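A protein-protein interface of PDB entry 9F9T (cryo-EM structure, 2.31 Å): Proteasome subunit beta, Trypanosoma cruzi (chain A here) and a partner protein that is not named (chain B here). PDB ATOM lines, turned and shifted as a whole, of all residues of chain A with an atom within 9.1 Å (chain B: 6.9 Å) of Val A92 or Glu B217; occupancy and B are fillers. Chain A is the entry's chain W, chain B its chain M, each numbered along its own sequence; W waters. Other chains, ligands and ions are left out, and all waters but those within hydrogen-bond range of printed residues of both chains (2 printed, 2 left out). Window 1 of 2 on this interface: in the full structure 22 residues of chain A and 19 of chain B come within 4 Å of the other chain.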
ATOM      1  N   THR A  84      16.424   7.054   2.754  1.00  0.00           N
ATOM      2  CA  THR A  84      17.466   7.218   3.734  1.00  0.00           C
ATOM      3  C   THR A  84      18.868   6.940   3.296  1.00  0.00           C
ATOM      4  O   THR A  84      19.713   7.038   4.152  1.00  0.00           O
ATOM      5  CB  THR A  84      17.255   6.341   4.951  1.00  0.00           C
ATOM      6  OG1 THR A  84      17.213   4.958   4.608  1.00  0.00           O
ATOM      7  CG2 THR A  84      15.947   6.728   5.618  1.00  0.00           C
ATOM      8  N   ARG A  85      19.174   6.797   2.031  1.00  0.00           N
ATOM      9  CA  ARG A  85      20.546   6.499   1.676  1.00  0.00           C
ATOM     10  C   ARG A  85      21.282   7.793   1.377  1.00  0.00           C
ATOM     11  O   ARG A  85      20.846   8.507   0.528  1.00  0.00           O
ATOM     12  CB  ARG A  85      20.552   5.571   0.467  1.00  0.00           C
ATOM     13  CG  ARG A  85      21.806   5.589  -0.395  1.00  0.00           C
ATOM     14  CD  ARG A  85      21.535   4.896  -1.741  1.00  0.00           C
ATOM     15  NE  ARG A  85      21.144   3.547  -1.423  1.00  0.00           N
ATOM     16  CZ  ARG A  85      21.035   2.612  -2.323  1.00  0.00           C
ATOM     17  NH1 ARG A  85      21.316   2.901  -3.578  1.00  0.00           N
ATOM     18  NH2 ARG A  85      20.567   1.436  -1.963  1.00  0.00           N
ATOM     19  N   ALA A  86      22.435   8.007   1.988  1.00  0.00           N
ATOM     20  CA  ALA A  86      23.423   8.978   1.555  1.00  0.00           C
ATOM     21  C   ALA A  86      24.618   8.295   0.899  1.00  0.00           C
ATOM     22  O   ALA A  86      25.205   7.366   1.472  1.00  0.00           O
ATOM     23  CB  ALA A  86      23.943   9.665   2.782  1.00  0.00           C
ATOM     24  N   THR A  87      25.092   8.871  -0.191  1.00  0.00           N
ATOM     25  CA  THR A  87      26.152   8.263  -0.974  1.00  0.00           C
ATOM     26  C   THR A  87      27.332   9.212  -1.113  1.00  0.00           C
ATOM     27  O   THR A  87      27.104  10.396  -1.325  1.00  0.00           O
ATOM     28  CB  THR A  87      25.661   7.962  -2.406  1.00  0.00           C
ATOM     29  OG1 THR A  87      25.013   9.127  -2.933  1.00  0.00           O
ATOM     30  CG2 THR A  87      24.668   6.816  -2.509  1.00  0.00           C
ATOM     31  N   GLU A  88      28.566   8.668  -1.167  1.00  0.00           N
ATOM     32  CA  GLU A  88      29.717   9.374  -1.737  1.00  0.00           C
ATOM     33  C   GLU A  88      30.212   8.693  -3.007  1.00  0.00           C
ATOM     34  O   GLU A  88      30.760   7.606  -2.985  1.00  0.00           O
ATOM     35  CB  GLU A  88      30.881   9.572  -0.756  1.00  0.00           C
ATOM     36  CG  GLU A  88      31.173   8.420   0.172  1.00  0.00           C
ATOM     37  CD  GLU A  88      31.615   8.860   1.565  1.00  0.00           C
ATOM     38  OE1 GLU A  88      31.323  10.021   1.955  1.00  0.00           O
ATOM     39  OE2 GLU A  88      32.264   8.042   2.266  1.00  0.00           O
ATOM     40  N   GLY A  89      30.032   9.364  -4.130  1.00  0.00           N
ATOM     41  CA  GLY A  89      30.309   8.731  -5.399  1.00  0.00           C
ATOM     42  C   GLY A  89      29.227   7.711  -5.748  1.00  0.00           C
ATOM     43  O   GLY A  89      28.110   8.053  -6.110  1.00  0.00           O
ATOM     44  N   SER A  90      29.614   6.448  -5.689  1.00  0.00           N
ATOM     45  CA  SER A  90      28.783   5.351  -6.132  1.00  0.00           C
ATOM     46  C   SER A  90      28.759   4.320  -5.014  1.00  0.00           C
ATOM     47  O   SER A  90      28.311   3.199  -5.215  1.00  0.00           O
ATOM     48  CB  SER A  90      29.301   4.810  -7.425  1.00  0.00           C
ATOM     49  OG  SER A  90      30.222   3.781  -7.154  1.00  0.00           O
ATOM     50  N   ILE A  91      29.149   4.793  -3.818  1.00  0.00           N
ATOM     51  CA  ILE A  91      29.208   3.976  -2.621  1.00  0.00           C
ATOM     52  C   ILE A  91      28.252   4.521  -1.582  1.00  0.00           C
ATOM     53  O   ILE A  91      28.249   5.714  -1.310  1.00  0.00           O
ATOM     54  CB  ILE A  91      30.653   3.980  -2.083  1.00  0.00           C
ATOM     55  CG1 ILE A  91      31.589   3.274  -3.051  1.00  0.00           C
ATOM     56  CG2 ILE A  91      30.770   3.403  -0.659  1.00  0.00           C
ATOM     57  CD1 ILE A  91      32.922   4.024  -3.166  1.00  0.00           C
ATOM     58  N   VAL A  92      27.535   3.637  -0.929  1.00  0.00           N
ATOM     59  CA  VAL A  92      26.722   4.010   0.209  1.00  0.00           C
ATOM     60  C   VAL A  92      27.579   4.263   1.460  1.00  0.00           C
ATOM     61  O   VAL A  92      28.213   3.385   2.031  1.00  0.00           O
ATOM     62  CB  VAL A  92      25.669   2.932   0.431  1.00  0.00           C
ATOM     63  CG1 VAL A  92      24.681   3.284   1.541  1.00  0.00           C
ATOM     64  CG2 VAL A  92      24.943   2.704  -0.857  1.00  0.00           C
ATOM     65  N   ALA A  93      27.574   5.507   1.895  1.00  0.00           N
ATOM     66  CA  ALA A  93      28.288   5.960   3.079  1.00  0.00           C
ATOM     67  C   ALA A  93      27.462   5.724   4.328  1.00  0.00           C
ATOM     68  O   ALA A  93      27.976   5.402   5.396  1.00  0.00           O
ATOM     69  CB  ALA A  93      28.557   7.418   2.916  1.00  0.00           C
ATOM     70  N   ASP A  94      26.159   5.939   4.185  1.00  0.00           N
ATOM     71  CA  ASP A  94      25.239   5.765   5.301  1.00  0.00           C
ATOM     72  C   ASP A  94      23.892   5.340   4.756  1.00  0.00           C
ATOM     73  O   ASP A  94      23.293   6.035   3.961  1.00  0.00           O
ATOM     74  CB  ASP A  94      25.134   7.056   6.147  1.00  0.00           C
ATOM     75  CG  ASP A  94      24.221   6.838   7.323  1.00  0.00           C
ATOM     76  OD1 ASP A  94      23.810   5.651   7.561  1.00  0.00           O
ATOM     77  OD2 ASP A  94      23.867   7.822   7.962  1.00  0.00           O
ATOM     78  N   LYS A  95      23.437   4.222   5.270  1.00  0.00           N
ATOM     79  CA  LYS A  95      22.219   3.599   4.846  1.00  0.00           C
ATOM     80  C   LYS A  95      21.012   4.247   5.512  1.00  0.00           C
ATOM     81  O   LYS A  95      19.931   4.164   4.928  1.00  0.00           O
ATOM     82  CB  LYS A  95      22.233   2.123   5.236  1.00  0.00           C
ATOM     83  CG  LYS A  95      23.229   1.290   4.451  1.00  0.00           C
ATOM     84  CD  LYS A  95      23.104  -0.188   4.740  1.00  0.00           C
ATOM     85  CE  LYS A  95      24.315  -0.722   5.477  1.00  0.00           C
ATOM     86  NZ  LYS A  95      23.926  -1.345   6.770  1.00  0.00           N
ATOM     87  N   ARG A  96      21.183   4.796   6.725  1.00  0.00           N
ATOM     88  CA  ARG A  96      20.071   5.229   7.551  1.00  0.00           C
ATOM     89  C   ARG A  96      20.221   6.689   7.921  1.00  0.00           C
ATOM     90  O   ARG A  96      19.950   7.129   9.025  1.00  0.00           O
ATOM     91  CB  ARG A  96      19.933   4.325   8.761  1.00  0.00           C
ATOM     92  CG  ARG A  96      18.906   3.219   8.539  1.00  0.00           C
ATOM     93  CD  ARG A  96      18.876   2.218   9.689  1.00  0.00           C
ATOM     94  NE  ARG A  96      19.875   1.166   9.500  1.00  0.00           N
ATOM     95  CZ  ARG A  96      19.704   0.100   8.721  1.00  0.00           C
ATOM     96  NH1 ARG A  96      20.714  -0.722   8.499  1.00  0.00           N
ATOM     97  NH2 ARG A  96      18.540  -0.118   8.122  1.00  0.00           N
ATOM     98  N   CYS A  97      20.563   7.476   6.931  1.00  0.00           N
ATOM     99  CA  CYS A  97      20.668   8.891   7.168  1.00  0.00           C
ATOM    100  C   CYS A  97      19.285   9.557   7.236  1.00  0.00           C
ATOM    101  O   CYS A  97      18.317   9.077   6.647  1.00  0.00           O
ATOM    102  CB  CYS A  97      21.573   9.411   6.080  1.00  0.00           C
ATOM    103  SG  CYS A  97      21.138  11.093   5.634  1.00  0.00           S
ATOM    104  N   PRO A 233      19.084   4.728  -8.541  1.00  0.00           N
ATOM    105  CA  PRO A 233      20.232   4.188  -7.828  1.00  0.00           C
ATOM    106  C   PRO A 233      20.791   5.048  -6.730  1.00  0.00           C
ATOM    107  O   PRO A 233      21.375   4.532  -5.798  1.00  0.00           O
ATOM    108  CB  PRO A 233      21.306   4.053  -8.909  1.00  0.00           C
ATOM    109  CG  PRO A 233      20.841   4.849 -10.124  1.00  0.00           C
ATOM    110  CD  PRO A 233      19.348   4.951  -9.982  1.00  0.00           C
ATOM    111  N   TYR A 234      20.543   6.340  -6.792  1.00  0.00           N
ATOM    112  CA  TYR A 234      20.963   7.211  -5.729  1.00  0.00           C
ATOM    113  C   TYR A 234      19.933   7.283  -4.603  1.00  0.00           C
ATOM    114  O   TYR A 234      20.088   8.158  -3.777  1.00  0.00           O
ATOM    115  CB  TYR A 234      21.243   8.633  -6.236  1.00  0.00           C
ATOM    116  CG  TYR A 234      22.442   8.639  -7.166  1.00  0.00           C
ATOM    117  CD1 TYR A 234      23.734   8.582  -6.682  1.00  0.00           C
ATOM    118  CD2 TYR A 234      22.255   8.461  -8.519  1.00  0.00           C
ATOM    119  CE1 TYR A 234      24.820   8.508  -7.540  1.00  0.00           C
ATOM    120  CE2 TYR A 234      23.326   8.369  -9.391  1.00  0.00           C
ATOM    121  CZ  TYR A 234      24.625   8.373  -8.908  1.00  0.00           C
ATOM    122  OH  TYR A 234      25.645   8.252  -9.833  1.00  0.00           O
ATOM    123  N   SER A 235      18.933   6.431  -4.535  1.00  0.00           N
ATOM    124  CA  SER A 235      18.021   6.492  -3.427  1.00  0.00           C
ATOM    125  C   SER A 235      17.857   5.088  -2.905  1.00  0.00           C
ATOM    126  O   SER A 235      17.799   4.167  -3.692  1.00  0.00           O
ATOM    127  CB  SER A 235      16.627   7.061  -3.843  1.00  0.00           C
ATOM    128  OG  SER A 235      16.697   8.400  -4.356  1.00  0.00           O
ATOM    129  N   GLY A 236      17.649   4.912  -1.628  1.00  0.00           N
ATOM    130  CA  GLY A 236      17.538   3.545  -1.175  1.00  0.00           C
ATOM    131  C   GLY A 236      17.162   3.433   0.294  1.00  0.00           C
ATOM    132  O   GLY A 236      16.924   4.407   0.970  1.00  0.00           O
ATOM    133  N   THR A 237      16.998   2.171   0.689  1.00  0.00           N
ATOM    134  CA  THR A 237      16.959   1.664   2.052  1.00  0.00           C
ATOM    135  C   THR A 237      15.558   1.622   2.642  1.00  0.00           C
ATOM    136  O   THR A 237      14.989   0.563   2.721  1.00  0.00           O
ATOM    137  CB  THR A 237      17.960   2.353   2.959  1.00  0.00           C
ATOM    138  OG1 THR A 237      19.302   2.245   2.507  1.00  0.00           O
ATOM    139  CG2 THR A 237      17.925   1.693   4.313  1.00  0.00           C
ATOM    140  N   ASN A 259      13.437  -3.500   2.405  1.00  0.00           N
ATOM    141  CA  ASN A 259      14.692  -4.200   2.141  1.00  0.00           C
ATOM    142  C   ASN A 259      15.335  -4.701   3.434  1.00  0.00           C
ATOM    143  O   ASN A 259      16.352  -4.159   3.867  1.00  0.00           O
ATOM    144  CB  ASN A 259      15.703  -3.296   1.426  1.00  0.00           C
ATOM    145  CG  ASN A 259      15.337  -2.960  -0.007  1.00  0.00           C
ATOM    146  OD1 ASN A 259      15.519  -3.775  -0.917  1.00  0.00           O
ATOM    147  ND2 ASN A 259      14.870  -1.736  -0.212  1.00  0.00           N
ATOM    148  N   GLU A 260      14.776  -5.764   4.024  1.00  0.00           N
ATOM    149  CA  GLU A 260      15.441  -6.464   5.118  1.00  0.00           C
ATOM    150  C   GLU A 260      16.327  -7.586   4.579  1.00  0.00           C
ATOM    151  O   GLU A 260      16.248  -7.945   3.404  1.00  0.00           O
ATOM    152  CB  GLU A 260      14.428  -7.024   6.124  1.00  0.00           C
ATOM    153  CG  GLU A 260      14.535  -6.386   7.502  1.00  0.00           C
ATOM    154  CD  GLU A 260      14.303  -4.888   7.515  1.00  0.00           C
ATOM    155  OE1 GLU A 260      15.267  -4.127   7.768  1.00  0.00           O
ATOM    156  OE2 GLU A 260      13.148  -4.490   7.270  1.00  0.00           O
ATOM    157  N   ARG A 261      17.148  -8.146   5.481  1.00  0.00           N
ATOM    158  CA  ARG A 261      18.132  -9.167   5.154  1.00  0.00           C
ATOM    159  C   ARG A 261      17.443 -10.500   4.821  1.00  0.00           C
ATOM    160  O   ARG A 261      16.305 -10.744   5.222  1.00  0.00           O
ATOM    161  CB  ARG A 261      19.158  -9.252   6.295  1.00  0.00           C
ATOM    162  CG  ARG A 261      20.479  -8.546   6.015  1.00  0.00           C
ATOM    163  CD  ARG A 261      21.451  -9.519   5.365  1.00  0.00           C
ATOM    164  NE  ARG A 261      22.634  -8.929   4.750  1.00  0.00           N
ATOM    165  CZ  ARG A 261      23.612  -8.316   5.405  1.00  0.00           C
ATOM    166  NH1 ARG A 261      23.474  -8.034   6.688  1.00  0.00           N
ATOM    167  NH2 ARG A 261      24.719  -7.968   4.768  1.00  0.00           N
ATOM    168  N   LYS A 262      18.165 -11.345   4.060  1.00  0.00           N
ATOM    169  CA  LYS A 262      17.673 -12.614   3.533  1.00  0.00           C
ATOM    170  C   LYS A 262      18.631 -13.734   3.960  1.00  0.00           C
ATOM    171  O   LYS A 262      18.245 -14.623   4.720  1.00  0.00           O
ATOM    172  CB  LYS A 262      17.554 -12.550   2.000  1.00  0.00           C
ATOM    173  CG  LYS A 262      17.452 -11.151   1.398  1.00  0.00           C
ATOM    174  CD  LYS A 262      17.269 -11.118  -0.113  1.00  0.00           C
ATOM    175  CE  LYS A 262      16.798  -9.766  -0.608  1.00  0.00           C
ATOM    176  NZ  LYS A 262      16.320  -9.800  -2.009  1.00  0.00           N
ATOM    177  N   TYR A 263      19.872 -13.681   3.444  1.00  0.00           N
ATOM    178  CA  TYR A 263      20.984 -14.523   3.873  1.00  0.00           C
ATOM    179  C   TYR A 263      21.572 -13.870   5.127  1.00  0.00           C
ATOM    180  O   TYR A 263      22.190 -12.810   5.018  1.00  0.00           O
ATOM    181  CB  TYR A 263      21.962 -14.624   2.681  1.00  0.00           C
ATOM    182  CG  TYR A 263      23.104 -15.648   2.688  1.00  0.00           C
ATOM    183  CD1 TYR A 263      22.865 -17.012   2.477  1.00  0.00           C
ATOM    184  CD2 TYR A 263      24.440 -15.252   2.836  1.00  0.00           C
ATOM    185  CE1 TYR A 263      23.899 -17.942   2.458  1.00  0.00           C
ATOM    186  CE2 TYR A 263      25.480 -16.176   2.822  1.00  0.00           C
ATOM    187  CZ  TYR A 263      25.209 -17.523   2.632  1.00  0.00           C
ATOM    188  OH  TYR A 263      26.226 -18.437   2.609  1.00  0.00           O
ATOM    189  N   LYS A 265      24.120 -12.689   7.755  1.00  0.00           N
ATOM    190  CA  LYS A 265      25.535 -12.483   7.479  1.00  0.00           C
ATOM    191  C   LYS A 265      26.351 -13.658   8.019  1.00  0.00           C
ATOM    192  O   LYS A 265      26.063 -14.175   9.096  1.00  0.00           O
ATOM    193  CB  LYS A 265      25.969 -11.142   8.088  1.00  0.00           C
ATOM    194  CG  LYS A 265      27.463 -10.837   8.063  1.00  0.00           C
ATOM    195  CD  LYS A 265      27.794  -9.359   8.192  1.00  0.00           C
ATOM    196  CE  LYS A 265      27.318  -8.742   9.492  1.00  0.00           C
ATOM    197  NZ  LYS A 265      27.610  -7.289   9.533  1.00  0.00           N
ATOM    198  N   PHE B 177      36.304  -2.944  -3.591  1.00  0.00           N
ATOM    199  CA  PHE B 177      36.200  -3.454  -2.248  1.00  0.00           C
ATOM    200  C   PHE B 177      36.121  -4.964  -2.142  1.00  0.00           C
ATOM    201  O   PHE B 177      36.374  -5.488  -1.053  1.00  0.00           O
ATOM    202  CB  PHE B 177      34.877  -3.436  -1.491  1.00  0.00           C
ATOM    203  CG  PHE B 177      33.679  -2.737  -2.028  1.00  0.00           C
ATOM    204  CD1 PHE B 177      33.759  -1.427  -2.380  1.00  0.00           C
ATOM    205  CD2 PHE B 177      32.458  -3.330  -1.900  1.00  0.00           C
ATOM    206  CE1 PHE B 177      32.650  -0.745  -2.809  1.00  0.00           C
ATOM    207  CE2 PHE B 177      31.341  -2.660  -2.351  1.00  0.00           C
ATOM    208  CZ  PHE B 177      31.453  -1.378  -2.826  1.00  0.00           C
ATOM    209  N   PHE B 212      29.523 -10.858  -2.496  1.00  0.00           N
ATOM    210  CA  PHE B 212      28.500 -10.205  -3.300  1.00  0.00           C
ATOM    211  C   PHE B 212      27.432  -9.556  -2.451  1.00  0.00           C
ATOM    212  O   PHE B 212      26.997  -8.459  -2.762  1.00  0.00           O
ATOM    213  CB  PHE B 212      27.821 -11.258  -4.154  1.00  0.00           C
ATOM    214  CG  PHE B 212      28.550 -11.437  -5.441  1.00  0.00           C
ATOM    215  CD1 PHE B 212      28.412 -10.493  -6.433  1.00  0.00           C
ATOM    216  CD2 PHE B 212      29.459 -12.459  -5.605  1.00  0.00           C
ATOM    217  CE1 PHE B 212      29.109 -10.625  -7.632  1.00  0.00           C
ATOM    218  CE2 PHE B 212      30.166 -12.593  -6.791  1.00  0.00           C
ATOM    219  CZ  PHE B 212      29.972 -11.699  -7.821  1.00  0.00           C
ATOM    220  N   THR B 213      27.006 -10.207  -1.380  1.00  0.00           N
ATOM    221  CA  THR B 213      26.060  -9.584  -0.484  1.00  0.00           C
ATOM    222  C   THR B 213      26.566  -8.228   0.015  1.00  0.00           C
ATOM    223  O   THR B 213      25.845  -7.249  -0.095  1.00  0.00           O
ATOM    224  CB  THR B 213      25.756 -10.476   0.711  1.00  0.00           C
ATOM    225  OG1 THR B 213      25.066 -11.653   0.308  1.00  0.00           O
ATOM    226  CG2 THR B 213      24.878  -9.775   1.717  1.00  0.00           C
ATOM    227  N   GLY B 214      27.814  -8.123   0.486  1.00  0.00           N
ATOM    228  CA  GLY B 214      28.424  -6.867   0.920  1.00  0.00           C
ATOM    229  C   GLY B 214      28.571  -5.868  -0.215  1.00  0.00           C
ATOM    230  O   GLY B 214      28.338  -4.680  -0.028  1.00  0.00           O
ATOM    231  N   ALA B 215      28.931  -6.330  -1.420  1.00  0.00           N
ATOM    232  CA  ALA B 215      29.010  -5.456  -2.587  1.00  0.00           C
ATOM    233  C   ALA B 215      27.676  -4.810  -2.912  1.00  0.00           C
ATOM    234  O   ALA B 215      27.627  -3.650  -3.256  1.00  0.00           O
ATOM    235  CB  ALA B 215      29.444  -6.212  -3.777  1.00  0.00           C
ATOM    236  N   ALA B 216      26.590  -5.553  -2.729  1.00  0.00           N
ATOM    237  CA  ALA B 216      25.300  -5.022  -3.100  1.00  0.00           C
ATOM    238  C   ALA B 216      24.883  -4.005  -2.062  1.00  0.00           C
ATOM    239  O   ALA B 216      24.401  -2.976  -2.444  1.00  0.00           O
ATOM    240  CB  ALA B 216      24.251  -6.111  -3.359  1.00  0.00           C
ATOM    241  N   GLU B 217      25.111  -4.243  -0.790  1.00  0.00           N
ATOM    242  CA  GLU B 217      24.819  -3.246   0.241  1.00  0.00           C
ATOM    243  C   GLU B 217      25.449  -1.871  -0.024  1.00  0.00           C
ATOM    244  O   GLU B 217      24.785  -0.879   0.147  1.00  0.00           O
ATOM    245  CB  GLU B 217      25.315  -3.734   1.604  1.00  0.00           C
ATOM    246  CG  GLU B 217      24.411  -4.785   2.210  1.00  0.00           C
ATOM    247  CD  GLU B 217      23.301  -4.233   3.082  1.00  0.00           C
ATOM    248  OE1 GLU B 217      22.256  -4.937   3.260  1.00  0.00           O
ATOM    249  OE2 GLU B 217      23.513  -3.123   3.623  1.00  0.00           O
ATOM    250  N   ARG B 218      26.669  -1.815  -0.502  1.00  0.00           N
ATOM    251  CA  ARG B 218      27.403  -0.582  -0.610  1.00  0.00           C
ATOM    252  C   ARG B 218      27.585  -0.068  -2.035  1.00  0.00           C
ATOM    253  O   ARG B 218      27.869   1.107  -2.181  1.00  0.00           O
ATOM    254  CB  ARG B 218      28.802  -0.816  -0.012  1.00  0.00           C
ATOM    255  CG  ARG B 218      28.727  -1.229   1.469  1.00  0.00           C
ATOM    256  CD  ARG B 218      28.524  -0.046   2.349  1.00  0.00           C
ATOM    257  NE  ARG B 218      28.151  -0.345   3.713  1.00  0.00           N
ATOM    258  CZ  ARG B 218      27.984   0.607   4.648  1.00  0.00           C
ATOM    259  NH1 ARG B 218      28.188   1.895   4.380  1.00  0.00           N
ATOM    260  NH2 ARG B 218      27.716   0.257   5.886  1.00  0.00           N
ATOM    261  N   ASP B 219      27.605  -0.921  -3.069  1.00  0.00           N
ATOM    262  CA  ASP B 219      27.829  -0.379  -4.390  1.00  0.00           C
ATOM    263  C   ASP B 219      26.463  -0.164  -5.061  1.00  0.00           C
ATOM    264  O   ASP B 219      25.716  -1.122  -5.268  1.00  0.00           O
ATOM    265  CB  ASP B 219      28.741  -1.235  -5.250  1.00  0.00           C
ATOM    266  CG  ASP B 219      28.734  -0.730  -6.703  1.00  0.00           C
ATOM    267  OD1 ASP B 219      28.977   0.546  -6.949  1.00  0.00           O
ATOM    268  OD2 ASP B 219      28.450  -1.549  -7.619  1.00  0.00           O
ATOM    269  N   ILE B 220      26.122   1.080  -5.405  1.00  0.00           N
ATOM    270  CA  ILE B 220      24.771   1.299  -5.858  1.00  0.00           C
ATOM    271  C   ILE B 220      24.511   0.690  -7.251  1.00  0.00           C
ATOM    272  O   ILE B 220      23.372   0.554  -7.651  1.00  0.00           O
ATOM    273  CB  ILE B 220      24.410   2.792  -5.950  1.00  0.00           C
ATOM    274  CG1 ILE B 220      25.206   3.423  -7.078  1.00  0.00           C
ATOM    275  CG2 ILE B 220      24.469   3.583  -4.643  1.00  0.00           C
ATOM    276  CD1 ILE B 220      25.097   4.931  -7.036  1.00  0.00           C
ATOM    277  N   THR B 222      25.355  -2.411  -8.224  1.00  0.00           N
ATOM    278  CA  THR B 222      25.505  -3.845  -8.159  1.00  0.00           C
ATOM    279  C   THR B 222      24.344  -4.356  -7.331  1.00  0.00           C
ATOM    280  O   THR B 222      24.105  -3.827  -6.246  1.00  0.00           O
ATOM    281  CB  THR B 222      26.861  -4.288  -7.543  1.00  0.00           C
ATOM    282  OG1 THR B 222      27.964  -4.072  -8.428  1.00  0.00           O
ATOM    283  CG2 THR B 222      26.902  -5.768  -7.199  1.00  0.00           C
ATOM    284  N   ARG B 244      20.091  -7.709  -2.469  1.00  0.00           N
ATOM    285  CA  ARG B 244      19.288  -6.510  -2.393  1.00  0.00           C
ATOM    286  C   ARG B 244      18.767  -6.007  -3.751  1.00  0.00           C
ATOM    287  O   ARG B 244      19.524  -5.835  -4.703  1.00  0.00           O
ATOM    288  CB  ARG B 244      20.064  -5.433  -1.646  1.00  0.00           C
ATOM    289  CG  ARG B 244      19.480  -5.224  -0.256  1.00  0.00           C
ATOM    290  CD  ARG B 244      20.321  -4.259   0.515  1.00  0.00           C
ATOM    291  NE  ARG B 244      19.845  -2.903   0.492  1.00  0.00           N
ATOM    292  CZ  ARG B 244      19.565  -2.218   1.594  1.00  0.00           C
ATOM    293  NH1 ARG B 244      19.491  -0.895   1.559  1.00  0.00           N
ATOM    294  NH2 ARG B 244      19.480  -2.856   2.749  1.00  0.00           N
ATOM    295  N   ASP B 246      17.276  -2.790  -3.995  1.00  0.00           N
ATOM    296  CA  ASP B 246      17.207  -1.328  -4.051  1.00  0.00           C
ATOM    297  C   ASP B 246      18.450  -0.743  -4.750  1.00  0.00           C
ATOM    298  O   ASP B 246      19.093  -1.513  -5.506  1.00  0.00           O
ATOM    299  CB  ASP B 246      16.927  -0.704  -2.674  1.00  0.00           C
ATOM    300  CG  ASP B 246      18.034  -0.689  -1.634  1.00  0.00           C
ATOM    301  OD1 ASP B 246      19.219  -0.733  -2.026  1.00  0.00           O
ATOM    302  OD2 ASP B 246      17.698  -0.618  -0.420  1.00  0.00           O
ATOM    303  OXT ASP B 246      18.736   0.478  -4.530  1.00  0.00           O
HETATM  304  O   HOH W   1      21.062   1.752   0.845  1.00  0.00           O
HETATM  305  O   HOH W   2      27.805   2.803   7.071  1.00  0.00           O
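The backbone NH (N) of Ile B220 lies within hydrogen-bond range of the backbone carbonyl oxygen (O) of Ser A90 (3.1 Å).
The side-chain carboxylate (OD1) of Asp B219 is in hydrogen-bond range of the side-chain hydroxyl (OG) of Ser A90, at 3.5 Å.
The side-chain carboxylate of Asp B246 is in salt-bridge range of the guanidinium group of Arg A85 (2.6 Å).
The backbone carbonyl oxygen (O) of Val A92 lies within hydrogen-bond range of the guanidinium group (NH1) of Arg B218.
OG1 of Thr A237 sits at hydrogen-bond distance from NH1 of Arg B244.
OE2 of Glu B217 is in salt-bridge range of NZ of Lys A95 (3.6 Å).
OD2 of Asp B246 lies within hydrogen-bond range of N of Thr A237, 3.1 Å away.
ND2 of Asn A259 is in hydrogen-bond range of OD2 of Asp B246, at 3.0 Å.
NH1 of Arg A85 is in hydrogen-bond range of O of Pro A233 (2.8 Å).
The side-chain carboxylate (OD2) of Asp B219 is in hydrogen-bond range of the side-chain hydroxyl (OG1) of Thr B222, at 2.7 Å.
The side-chain hydroxyl (OG1) of Thr A84 sits at hydrogen-bond distance from the backbone carbonyl oxygen (O) of Lys A95 (2.8 Å).
NH2 of Arg B244 lies within salt-bridge range of OE1 of Glu B217, 3.5 Å away.
CG2 of Ile B220 touches NH1 of Arg A85, 3.4 Å away.
Thr A87 touches Ile B220 (CG2 to CG2, 3.9 Å).
CA of Ile A91 touches O of Arg B218 (3.2 Å).
CG2 of Val A92 touches O of Glu B217, at 3.7 Å.
Ile B220 touches Val A92.
Ala A93 touches Arg B218.
O of Pro A233 touches CG2 of Ile B220, at 3.4 Å.
Ser A235 touches Asp B246.
Asn A259 touches Arg B244.
CG2 of Thr B213 touches NH2 of Arg A261, 3.5 Å away.
Val A92 touches just these residues of chain B: Glu B217, Arg B218 and Ile B220.
Glu B217 touches just these residues of chain A: Val A92 (3.7 Å) and Lys A95 (3.1 Å).
No residue of chain A comes within 4 Å of Ala B216.
Arg B218 touches five residues of chain A.
Of the printed residues of chain B, Arg A85 touches Ile B220 and Asp B246.
Of the printed residues of chain B, Ser A235 touches Asp B246 (3.9 Å).
Printed residues of chain A within 4 Å of Arg B244: Thr A237 and Asn A259.
Of the printed residues of chain B, Arg A261 touches Thr B213.
Arg A96 touches none of the printed residues of chain B.
The nearest residue of chain B that does not touch Val A92 is Asp B219 (5.0 Å).
Of the 25 printed residues of chain A, 13 touch a printed residue of chain B.
Hydrophobic or aromatic side chains of chain A that line the printed part of chain B: Val A92 and Tyr A234.
Of the 13 printed residues of chain B, 7 touch a printed residue of chain A.
Printed residues of chain B that touch a printed residue of chain A: Thr B213, Glu B217, Arg B218, Asp B219, Ile B220, Arg B244 and Asp B246.
Hydrophobic or aromatic side chains of chain B within 4 Å of the printed part of chain A: Ile B220.
Among the printed residues, 21 pairs touch across the chains.
Among the printed residues, Asp or Glu carboxylates within 4 Å of a Lys or Arg side-chain nitrogen of the other chain: Arg A85 with Asp B246 (2.6 Å) and Lys A95 with Glu B217 (3.6 Å).
Water W1 lies within hydrogen-bond range of the side-chain hydroxyl of Thr A237 (2.5 Å), the guanidinium group of Arg A85 (2.9 Å) and the guanidinium group of Arg B244 (3.2 Å).
Water W2 bridges the guanidinium group (NH2) of Arg B218 and the backbone carbonyl oxygen (O) of Ala A93.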
